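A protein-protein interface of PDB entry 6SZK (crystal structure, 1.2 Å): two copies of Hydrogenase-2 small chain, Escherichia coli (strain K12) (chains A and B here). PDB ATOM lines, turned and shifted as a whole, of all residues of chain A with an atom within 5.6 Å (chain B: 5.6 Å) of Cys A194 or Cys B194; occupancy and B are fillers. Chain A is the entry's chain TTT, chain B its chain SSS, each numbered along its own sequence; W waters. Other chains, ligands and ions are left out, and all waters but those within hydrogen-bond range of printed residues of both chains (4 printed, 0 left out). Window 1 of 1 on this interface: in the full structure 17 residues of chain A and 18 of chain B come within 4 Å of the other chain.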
ATOM      1  N   ILE A 190     -26.868  12.445  -6.397  1.00  0.00           N
ATOM      2  CA  ILE A 190     -25.733  12.137  -5.488  1.00  0.00           C
ATOM      3  C   ILE A 190     -24.493  12.897  -5.995  1.00  0.00           C
ATOM      4  O   ILE A 190     -23.760  13.527  -5.152  1.00  0.00           O
ATOM      5  CB  ILE A 190     -25.535  10.607  -5.371  1.00  0.00           C
ATOM      6  CG1 ILE A 190     -26.705   9.972  -4.613  1.00  0.00           C
ATOM      7  CG2 ILE A 190     -24.176  10.268  -4.750  1.00  0.00           C
ATOM      8  CD1 ILE A 190     -26.748   8.443  -4.612  1.00  0.00           C
ATOM      9  N   HIS A 191     -24.207  12.894  -7.311  1.00  0.00           N
ATOM     10  CA  HIS A 191     -23.012  13.571  -7.890  1.00  0.00           C
ATOM     11  C   HIS A 191     -23.043  15.098  -7.737  1.00  0.00           C
ATOM     12  O   HIS A 191     -21.979  15.755  -7.821  1.00  0.00           O
ATOM     13  CB  HIS A 191     -22.923  13.157  -9.358  1.00  0.00           C
ATOM     14  CG  HIS A 191     -21.786  13.729 -10.154  1.00  0.00           C
ATOM     15  ND1 HIS A 191     -20.492  13.212 -10.104  1.00  0.00           N
ATOM     16  CD2 HIS A 191     -21.765  14.704 -11.121  1.00  0.00           C
ATOM     17  CE1 HIS A 191     -19.764  13.905 -10.961  1.00  0.00           C
ATOM     18  NE2 HIS A 191     -20.508  14.796 -11.613  1.00  0.00           N
ATOM     19  N   GLU A 192     -24.249  15.662  -7.505  1.00  0.00           N
ATOM     20  CA  GLU A 192     -24.377  17.118  -7.252  1.00  0.00           C
ATOM     21  C   GLU A 192     -24.247  17.461  -5.743  1.00  0.00           C
ATOM     22  O   GLU A 192     -24.441  18.656  -5.386  1.00  0.00           O
ATOM     23  CB  GLU A 192     -25.655  17.683  -7.901  1.00  0.00           C
ATOM     24  CG  GLU A 192     -25.575  17.641  -9.440  1.00  0.00           C
ATOM     25  CD  GLU A 192     -24.403  18.406 -10.020  1.00  0.00           C
ATOM     26  OE1 GLU A 192     -24.242  19.615  -9.679  1.00  0.00           O
ATOM     27  OE2 GLU A 192     -23.607  17.873 -10.849  1.00  0.00           O
ATOM     28  N   HIS A 193     -23.847  16.497  -4.922  1.00  0.00           N
ATOM     29  CA  HIS A 193     -23.530  16.768  -3.499  1.00  0.00           C
ATOM     30  C   HIS A 193     -22.567  15.694  -2.968  1.00  0.00           C
ATOM     31  O   HIS A 193     -22.690  15.229  -1.800  1.00  0.00           O
ATOM     32  CB  HIS A 193     -24.837  16.876  -2.635  1.00  0.00           C
ATOM     33  CG  HIS A 193     -24.757  17.828  -1.461  1.00  0.00           C
ATOM     34  ND1 HIS A 193     -25.411  19.046  -1.451  1.00  0.00           N
ATOM     35  CD2 HIS A 193     -24.011  17.737  -0.303  1.00  0.00           C
ATOM     36  CE1 HIS A 193     -25.077  19.678  -0.286  1.00  0.00           C
ATOM     37  NE2 HIS A 193     -24.201  18.877   0.434  1.00  0.00           N
ATOM     38  N   CYS A 194     -21.584  15.313  -3.767  1.00  0.00           N
ATOM     39  CA  CYS A 194     -20.571  14.257  -3.454  1.00  0.00           C
ATOM     40  C   CYS A 194     -19.190  14.847  -3.103  1.00  0.00           C
ATOM     41  O   CYS A 194     -18.668  15.676  -3.857  1.00  0.00           O
ATOM     42  CB  CYS A 194     -20.399  13.266  -4.633  1.00  0.00           C
ATOM     43  SG  CYS A 194     -19.192  11.936  -4.251  1.00  0.00           S
ATOM     44  N   GLU A 195     -18.639  14.416  -1.960  1.00  0.00           N
ATOM     45  CA  GLU A 195     -17.340  14.885  -1.453  1.00  0.00           C
ATOM     46  C   GLU A 195     -16.194  14.545  -2.370  1.00  0.00           C
ATOM     47  O   GLU A 195     -15.074  15.097  -2.178  1.00  0.00           O
ATOM     48  CB  GLU A 195     -17.086  14.493   0.002  1.00  0.00           C
ATOM     49  CG  GLU A 195     -16.912  12.994   0.230  1.00  0.00           C
ATOM     50  CD  GLU A 195     -18.094  12.072   0.364  1.00  0.00           C
ATOM     51  OE1 GLU A 195     -19.263  12.480   0.020  1.00  0.00           O
ATOM     52  OE2 GLU A 195     -17.833  10.882   0.884  1.00  0.00           O
ATOM     53  N   ARG A 196     -16.369  13.608  -3.340  1.00  0.00           N
ATOM     54  CA  ARG A 196     -15.277  13.261  -4.280  1.00  0.00           C
ATOM     55  C   ARG A 196     -15.346  14.073  -5.596  1.00  0.00           C
ATOM     56  O   ARG A 196     -14.440  13.919  -6.473  1.00  0.00           O
ATOM     57  CB  ARG A 196     -15.162  11.754  -4.561  1.00  0.00           C
ATOM     58  CG  ARG A 196     -15.012  10.923  -3.282  1.00  0.00           C
ATOM     59  CD  ARG A 196     -14.586   9.523  -3.435  1.00  0.00           C
ATOM     60  NE  ARG A 196     -14.412   8.887  -2.140  1.00  0.00           N
ATOM     61  CZ  ARG A 196     -13.742   7.788  -1.919  1.00  0.00           C
ATOM     62  NH1 ARG A 196     -13.205   7.081  -2.948  1.00  0.00           N
ATOM     63  NH2 ARG A 196     -13.548   7.344  -0.683  1.00  0.00           N
ATOM     64  N   ARG A 197     -16.298  15.020  -5.705  1.00  0.00           N
ATOM     65  CA  ARG A 197     -16.414  15.896  -6.890  1.00  0.00           C
ATOM     66  C   ARG A 197     -15.063  16.604  -7.204  1.00  0.00           C
ATOM     67  O   ARG A 197     -14.726  16.759  -8.401  1.00  0.00           O
ATOM     68  CB  ARG A 197     -17.603  16.827  -6.769  1.00  0.00           C
ATOM     69  CG  ARG A 197     -17.756  17.747  -7.982  1.00  0.00           C
ATOM     70  CD  ARG A 197     -18.092  17.002  -9.275  1.00  0.00           C
ATOM     71  NE  ARG A 197     -18.455  17.935 -10.371  1.00  0.00           N
ATOM     72  CZ  ARG A 197     -19.663  18.408 -10.594  1.00  0.00           C
ATOM     73  NH1 ARG A 197     -20.753  17.880 -10.021  1.00  0.00           N
ATOM     74  NH2 ARG A 197     -19.815  19.444 -11.425  1.00  0.00           N
ATOM     75  N   PRO A 198     -14.306  17.134  -6.210  1.00  0.00           N
ATOM     76  CA  PRO A 198     -13.008  17.765  -6.579  1.00  0.00           C
ATOM     77  C   PRO A 198     -12.079  16.832  -7.401  1.00  0.00           C
ATOM     78  O   PRO A 198     -11.342  17.305  -8.310  1.00  0.00           O
ATOM     79  CB  PRO A 198     -12.365  18.110  -5.229  1.00  0.00           C
ATOM     80  CG  PRO A 198     -13.595  18.254  -4.257  1.00  0.00           C
ATOM     81  CD  PRO A 198     -14.535  17.168  -4.732  1.00  0.00           C
ATOM     82  N   SER A 235     -24.772  10.489   0.155  1.00  0.00           N
ATOM     83  CA  SER A 235     -23.493  11.165   0.475  1.00  0.00           C
ATOM     84  C   SER A 235     -23.605  12.053   1.719  1.00  0.00           C
ATOM     85  O   SER A 235     -22.532  12.394   2.296  1.00  0.00           O
ATOM     86  CB  SER A 235     -22.965  11.949  -0.712  1.00  0.00           C
ATOM     87  OG  SER A 235     -23.924  12.971  -1.044  1.00  0.00           O
ATOM     88  N   TRP A 246     -21.022   5.222   3.693  1.00  0.00           N
ATOM     89  CA  TRP A 246     -21.859   5.013   2.506  1.00  0.00           C
ATOM     90  C   TRP A 246     -21.000   4.300   1.470  1.00  0.00           C
ATOM     91  O   TRP A 246     -19.766   4.171   1.665  1.00  0.00           O
ATOM     92  CB  TRP A 246     -22.507   6.305   1.938  1.00  0.00           C
ATOM     93  CG  TRP A 246     -21.579   7.325   1.255  1.00  0.00           C
ATOM     94  CD1 TRP A 246     -20.671   8.204   1.853  1.00  0.00           C
ATOM     95  CD2 TRP A 246     -21.660   7.748  -0.129  1.00  0.00           C
ATOM     96  NE1 TRP A 246     -20.149   9.049   0.898  1.00  0.00           N
ATOM     97  CE2 TRP A 246     -20.748   8.821  -0.322  1.00  0.00           C
ATOM     98  CE3 TRP A 246     -22.409   7.315  -1.272  1.00  0.00           C
ATOM     99  CZ2 TRP A 246     -20.607   9.470  -1.564  1.00  0.00           C
ATOM    100  CZ3 TRP A 246     -22.322   7.976  -2.477  1.00  0.00           C
ATOM    101  CH2 TRP A 246     -21.409   9.052  -2.616  1.00  0.00           C
ATOM    102  N   VAL A 248     -19.609   4.708  -1.547  1.00  0.00           N
ATOM    103  CA  VAL A 248     -18.428   5.430  -2.137  1.00  0.00           C
ATOM    104  C   VAL A 248     -17.357   5.673  -1.072  1.00  0.00           C
ATOM    105  O   VAL A 248     -16.149   5.472  -1.308  1.00  0.00           O
ATOM    106  CB  VAL A 248     -18.908   6.730  -2.891  1.00  0.00           C
ATOM    107  CG1 VAL A 248     -17.725   7.681  -3.167  1.00  0.00           C
ATOM    108  CG2 VAL A 248     -19.664   6.339  -4.169  1.00  0.00           C
ATOM    109  N   ILE B 190      -9.464  20.933   2.599  1.00  0.00           N
ATOM    110  CA  ILE B 190     -10.912  20.692   2.814  1.00  0.00           C
ATOM    111  C   ILE B 190     -11.675  20.854   1.479  1.00  0.00           C
ATOM    112  O   ILE B 190     -12.520  19.963   1.128  1.00  0.00           O
ATOM    113  CB  ILE B 190     -11.472  21.556   3.967  1.00  0.00           C
ATOM    114  CG1 ILE B 190     -10.869  21.071   5.326  1.00  0.00           C
ATOM    115  CG2 ILE B 190     -12.993  21.556   3.997  1.00  0.00           C
ATOM    116  CD1 ILE B 190     -11.108  22.077   6.454  1.00  0.00           C
ATOM    117  N   HIS B 191     -11.377  21.888   0.676  1.00  0.00           N
ATOM    118  CA  HIS B 191     -12.071  22.143  -0.594  1.00  0.00           C
ATOM    119  C   HIS B 191     -11.786  21.065  -1.657  1.00  0.00           C
ATOM    120  O   HIS B 191     -12.586  20.983  -2.640  1.00  0.00           O
ATOM    121  CB  HIS B 191     -11.626  23.555  -1.078  1.00  0.00           C
ATOM    122  CG  HIS B 191     -12.203  24.071  -2.365  1.00  0.00           C
ATOM    123  ND1 HIS B 191     -13.498  24.575  -2.475  1.00  0.00           N
ATOM    124  CD2 HIS B 191     -11.643  24.201  -3.595  1.00  0.00           C
ATOM    125  CE1 HIS B 191     -13.680  24.986  -3.746  1.00  0.00           C
ATOM    126  NE2 HIS B 191     -12.553  24.758  -4.464  1.00  0.00           N
ATOM    127  N   GLU B 192     -10.688  20.335  -1.511  1.00  0.00           N
ATOM    128  CA  GLU B 192     -10.389  19.227  -2.416  1.00  0.00           C
ATOM    129  C   GLU B 192     -11.048  17.888  -1.961  1.00  0.00           C
ATOM    130  O   GLU B 192     -10.779  16.823  -2.597  1.00  0.00           O
ATOM    131  CB  GLU B 192      -8.867  19.071  -2.706  1.00  0.00           C
ATOM    132  CG  GLU B 192      -8.303  20.301  -3.447  1.00  0.00           C
ATOM    133  CD  GLU B 192      -8.963  20.559  -4.822  1.00  0.00           C
ATOM    134  OE1 GLU B 192      -9.447  21.697  -5.114  1.00  0.00           O
ATOM    135  OE2 GLU B 192      -9.066  19.599  -5.599  1.00  0.00           O
ATOM    136  N   HIS B 193     -11.923  17.932  -0.954  1.00  0.00           N
ATOM    137  CA  HIS B 193     -12.733  16.768  -0.550  1.00  0.00           C
ATOM    138  C   HIS B 193     -14.054  17.219   0.086  1.00  0.00           C
ATOM    139  O   HIS B 193     -14.505  16.574   1.059  1.00  0.00           O
ATOM    140  CB  HIS B 193     -11.932  15.755   0.307  1.00  0.00           C
ATOM    141  CG  HIS B 193     -12.276  14.313   0.131  1.00  0.00           C
ATOM    142  ND1 HIS B 193     -11.404  13.406  -0.531  1.00  0.00           N
ATOM    143  CD2 HIS B 193     -13.413  13.630   0.464  1.00  0.00           C
ATOM    144  CE1 HIS B 193     -12.040  12.224  -0.555  1.00  0.00           C
ATOM    145  NE2 HIS B 193     -13.290  12.321   0.065  1.00  0.00           N
ATOM    146  N   CYS B 194     -14.676  18.280  -0.436  1.00  0.00           N
ATOM    147  CA  CYS B 194     -15.918  18.875   0.139  1.00  0.00           C
ATOM    148  C   CYS B 194     -17.173  18.488  -0.671  1.00  0.00           C
ATOM    149  O   CYS B 194     -17.155  18.706  -1.931  1.00  0.00           O
ATOM    150  CB  CYS B 194     -15.790  20.409   0.191  1.00  0.00           C
ATOM    151  SG  CYS B 194     -17.294  21.189   0.924  1.00  0.00           S
ATOM    152  N   GLU B 195     -18.220  18.037  -0.018  1.00  0.00           N
ATOM    153  CA  GLU B 195     -19.451  17.644  -0.677  1.00  0.00           C
ATOM    154  C   GLU B 195     -20.227  18.798  -1.328  1.00  0.00           C
ATOM    155  O   GLU B 195     -21.171  18.531  -2.134  1.00  0.00           O
ATOM    156  CB  GLU B 195     -20.358  16.822   0.269  1.00  0.00           C
ATOM    157  CG  GLU B 195     -20.962  17.599   1.451  1.00  0.00           C
ATOM    158  CD  GLU B 195     -20.129  17.829   2.724  1.00  0.00           C
ATOM    159  OE1 GLU B 195     -18.865  17.620   2.722  1.00  0.00           O
ATOM    160  OE2 GLU B 195     -20.775  18.233   3.778  1.00  0.00           O
ATOM    161  N   ARG B 196     -19.843  20.065  -1.037  1.00  0.00           N
ATOM    162  CA  ARG B 196     -20.502  21.213  -1.693  1.00  0.00           C
ATOM    163  C   ARG B 196     -19.717  21.699  -2.930  1.00  0.00           C
ATOM    164  O   ARG B 196     -20.181  22.620  -3.640  1.00  0.00           O
ATOM    165  CB  ARG B 196     -20.759  22.358  -0.724  1.00  0.00           C
ATOM    166  CG  ARG B 196     -21.580  21.896   0.489  1.00  0.00           C
ATOM    167  CD  ARG B 196     -22.191  23.012   1.313  1.00  0.00           C
ATOM    168  NE  ARG B 196     -23.038  22.435   2.355  1.00  0.00           N
ATOM    169  CZ  ARG B 196     -23.958  23.094   3.041  1.00  0.00           C
ATOM    170  NH1 ARG B 196     -24.114  24.411   2.884  1.00  0.00           N
ATOM    171  NH2 ARG B 196     -24.711  22.465   3.927  1.00  0.00           N
ATOM    172  N   ARG B 197     -18.673  20.975  -3.324  1.00  0.00           N
ATOM    173  CA  ARG B 197     -17.920  21.379  -4.526  1.00  0.00           C
ATOM    174  C   ARG B 197     -18.802  21.413  -5.798  1.00  0.00           C
ATOM    175  O   ARG B 197     -18.585  22.303  -6.656  1.00  0.00           O
ATOM    176  CB  ARG B 197     -16.724  20.443  -4.726  1.00  0.00           C
ATOM    177  CG  ARG B 197     -15.813  20.746  -5.953  1.00  0.00           C
ATOM    178  CD  ARG B 197     -15.186  22.139  -5.913  1.00  0.00           C
ATOM    179  NE  ARG B 197     -14.276  22.310  -7.029  1.00  0.00           N
ATOM    180  CZ  ARG B 197     -12.981  21.934  -7.019  1.00  0.00           C
ATOM    181  NH1 ARG B 197     -12.378  21.600  -5.886  1.00  0.00           N
ATOM    182  NH2 ARG B 197     -12.280  21.908  -8.174  1.00  0.00           N
ATOM    183  N   PRO B 198     -19.800  20.504  -6.007  1.00  0.00           N
ATOM    184  CA  PRO B 198     -20.660  20.648  -7.200  1.00  0.00           C
ATOM    185  C   PRO B 198     -21.325  22.046  -7.265  1.00  0.00           C
ATOM    186  O   PRO B 198     -21.522  22.568  -8.396  1.00  0.00           O
ATOM    187  CB  PRO B 198     -21.690  19.505  -7.082  1.00  0.00           C
ATOM    188  CG  PRO B 198     -21.000  18.446  -6.178  1.00  0.00           C
ATOM    189  CD  PRO B 198     -20.182  19.297  -5.218  1.00  0.00           C
ATOM    190  N   SER B 235     -14.406  17.599   6.525  1.00  0.00           N
ATOM    191  CA  SER B 235     -15.516  17.192   5.661  1.00  0.00           C
ATOM    192  C   SER B 235     -15.763  15.681   5.639  1.00  0.00           C
ATOM    193  O   SER B 235     -16.887  15.260   5.251  1.00  0.00           O
ATOM    194  CB  SER B 235     -15.337  17.691   4.239  1.00  0.00           C
ATOM    195  OG  SER B 235     -14.132  17.144   3.689  1.00  0.00           O
ATOM    196  N   TRP B 246     -20.243  18.907  10.804  1.00  0.00           N
ATOM    197  CA  TRP B 246     -19.048  19.780  10.712  1.00  0.00           C
ATOM    198  C   TRP B 246     -19.557  21.161  10.395  1.00  0.00           C
ATOM    199  O   TRP B 246     -20.777  21.363  10.073  1.00  0.00           O
ATOM    200  CB  TRP B 246     -17.980  19.267   9.698  1.00  0.00           C
ATOM    201  CG  TRP B 246     -18.322  19.353   8.213  1.00  0.00           C
ATOM    202  CD1 TRP B 246     -19.227  18.585   7.481  1.00  0.00           C
ATOM    203  CD2 TRP B 246     -17.615  20.136   7.210  1.00  0.00           C
ATOM    204  NE1 TRP B 246     -19.107  18.858   6.123  1.00  0.00           N
ATOM    205  CE2 TRP B 246     -18.141  19.800   5.923  1.00  0.00           C
ATOM    206  CE3 TRP B 246     -16.537  21.091   7.278  1.00  0.00           C
ATOM    207  CZ2 TRP B 246     -17.634  20.369   4.725  1.00  0.00           C
ATOM    208  CZ3 TRP B 246     -16.049  21.614   6.127  1.00  0.00           C
ATOM    209  CH2 TRP B 246     -16.569  21.235   4.863  1.00  0.00           C
ATOM    210  N   VAL B 248     -19.502  23.486   7.981  1.00  0.00           N
ATOM    211  CA  VAL B 248     -20.139  23.755   6.657  1.00  0.00           C
ATOM    212  C   VAL B 248     -21.471  22.993   6.564  1.00  0.00           C
ATOM    213  O   VAL B 248     -22.502  23.543   6.117  1.00  0.00           O
ATOM    214  CB  VAL B 248     -19.183  23.406   5.519  1.00  0.00           C
ATOM    215  CG1 VAL B 248     -19.916  23.301   4.156  1.00  0.00           C
ATOM    216  CG2 VAL B 248     -18.073  24.454   5.392  1.00  0.00           C
HETATM  217  O   HOH W   1     -15.183  10.075   0.523  1.00  0.00           O
HETATM  218  O   HOH W   2     -22.216  21.037 -10.716  1.00  0.00           O
HETATM  219  O   HOH W   3     -23.162  19.521   3.148  1.00  0.00           O
HETATM  220  O   HOH W   4     -10.111  19.861  -8.077  1.00  0.00           O
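Water W2 lies within hydrogen-bond range of the side-chain carboxylate of Glu A192 (2.7 Å), the backbone carbonyl oxygen of Pro B198 (2.9 Å) and the guanidinium group of Arg A197 (3.0 Å).
Water W4 lies within hydrogen-bond range of the side-chain carboxylate of Glu B192 (2.7 Å), the backbone carbonyl oxygen of Pro A198 (2.8 Å) and the guanidinium group of Arg B197 (3.0 Å).
Water W3 lies within hydrogen-bond range of the side-chain carboxylate (OE2) of Glu B195 (2.8 Å), a ring nitrogen (NE2) of His A193 (3.0 Å) and the guanidinium group (NE) of Arg B196 (3.0 Å).
Water W1 lies within hydrogen-bond range of OE2 of Glu A195 (2.8 Å), NE2 of His B193 (3.0 Å) and NE of Arg A196 (3.0 Å).
The side-chain hydroxyl (OG) of Ser A235 is in hydrogen-bond range of the backbone carbonyl oxygen (O) of His A193.
The side-chain carboxylate (OE1) of Glu B192 is in salt-bridge range of the guanidinium group (NH1) of Arg B197, 3.0 Å away.
N of Arg B196 lies close to SG of Cys B194.
The indole nitrogen (NE1) of Trp B246 is in hydrogen-bond range of the side-chain carboxylate (OE2) of Glu B195, 2.9 Å away.
The side-chain sulfur (SG) of Cys A194 lies close to the backbone NH (N) of Arg A196.
The guanidinium group (NH1) of Arg A197 lies within salt-bridge range of the side-chain carboxylate (OE2) of Glu A192 (3.0 Å).
Of the printed residues of chain B, His A191 touches Pro B198.
Of the printed residues of chain B, Glu A192 touches Pro B198 (3.3 Å).
Printed residues of chain B within 4 Å of Cys A194: Cys B194 (3.9 Å), Glu B195 (3.6 Å) and Pro B198 (3.996 Å).
Printed residues of chain A within 4 Å of Glu B192: Pro A198.
Of chain A, only Cys A194 (3.9 Å), Glu A195 (3.7 Å) and Pro A198 (3.97 Å) come within 4 Å of Cys B194.
Printed residues of chain A within 4 Å of Glu B195: His A193 (3.2 Å), Cys A194 (3.6 Å) and Glu A195 (3.6 Å).
Among the printed residues, merely in contact across the chains: His A193 with Glu B195 (3.2 Å), Glu A195 with His B193 (3.3 Å), His A191 with Pro B198 (3.3 Å), Pro A198 with His B191 (3.3 Å), Pro A198 with Glu B192 (3.3 Å), Glu A192 with Pro B198 (3.3 Å), Arg A197 with Pro B198 (3.5 Å), Pro A198 with Arg B197 (3.6 Å), Glu A195 with Glu B195 (3.6 Å), Cys A194 with Glu B195 (3.6 Å), Glu A195 with Cys B194 (3.7 Å), His A193 with Pro B198 (3.7 Å), Pro A198 with His B193 (3.7 Å), Cys A194 with Cys B194 (3.9 Å), Pro A198 with Cys B194 (3.97 Å), Cys A194 with Pro B198 (3.996 Å) and His A193 with Arg B196 (3.998 Å).
Of the 12 printed residues of chain B, 8 touch a printed residue of chain A.
Printed residues of chain B that touch a printed residue of chain A: His B191, Glu B192, His B193, Cys B194, Glu B195, Arg B196, Arg B197 and Pro B198.
Printed residues of chain A that touch a printed residue of chain B: His A191, Glu A192, His A193, Cys A194, Glu A195, Arg A197 and Pro A198.
Hydrophobic or aromatic side chains of chain A within 4 Å of the printed part of chain B: His A193 and Pro A198.
Among the printed residues, no Asp or Glu carboxylate lies within 4 Å of a Lys or Arg side-chain nitrogen of the other chain.
His A193 touches Glu B195, and with the chains exchanged Glu A195 touches His B193.
Cys A194 touches its own counterpart, Cys B194.
Cys A194 touches Glu B195, and with the chains exchanged Glu A195 touches Cys B194.
Cys A194 touches Pro B198, and with the chains exchanged Pro A198 touches Cys B194.
12 positions are printed for both chains.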
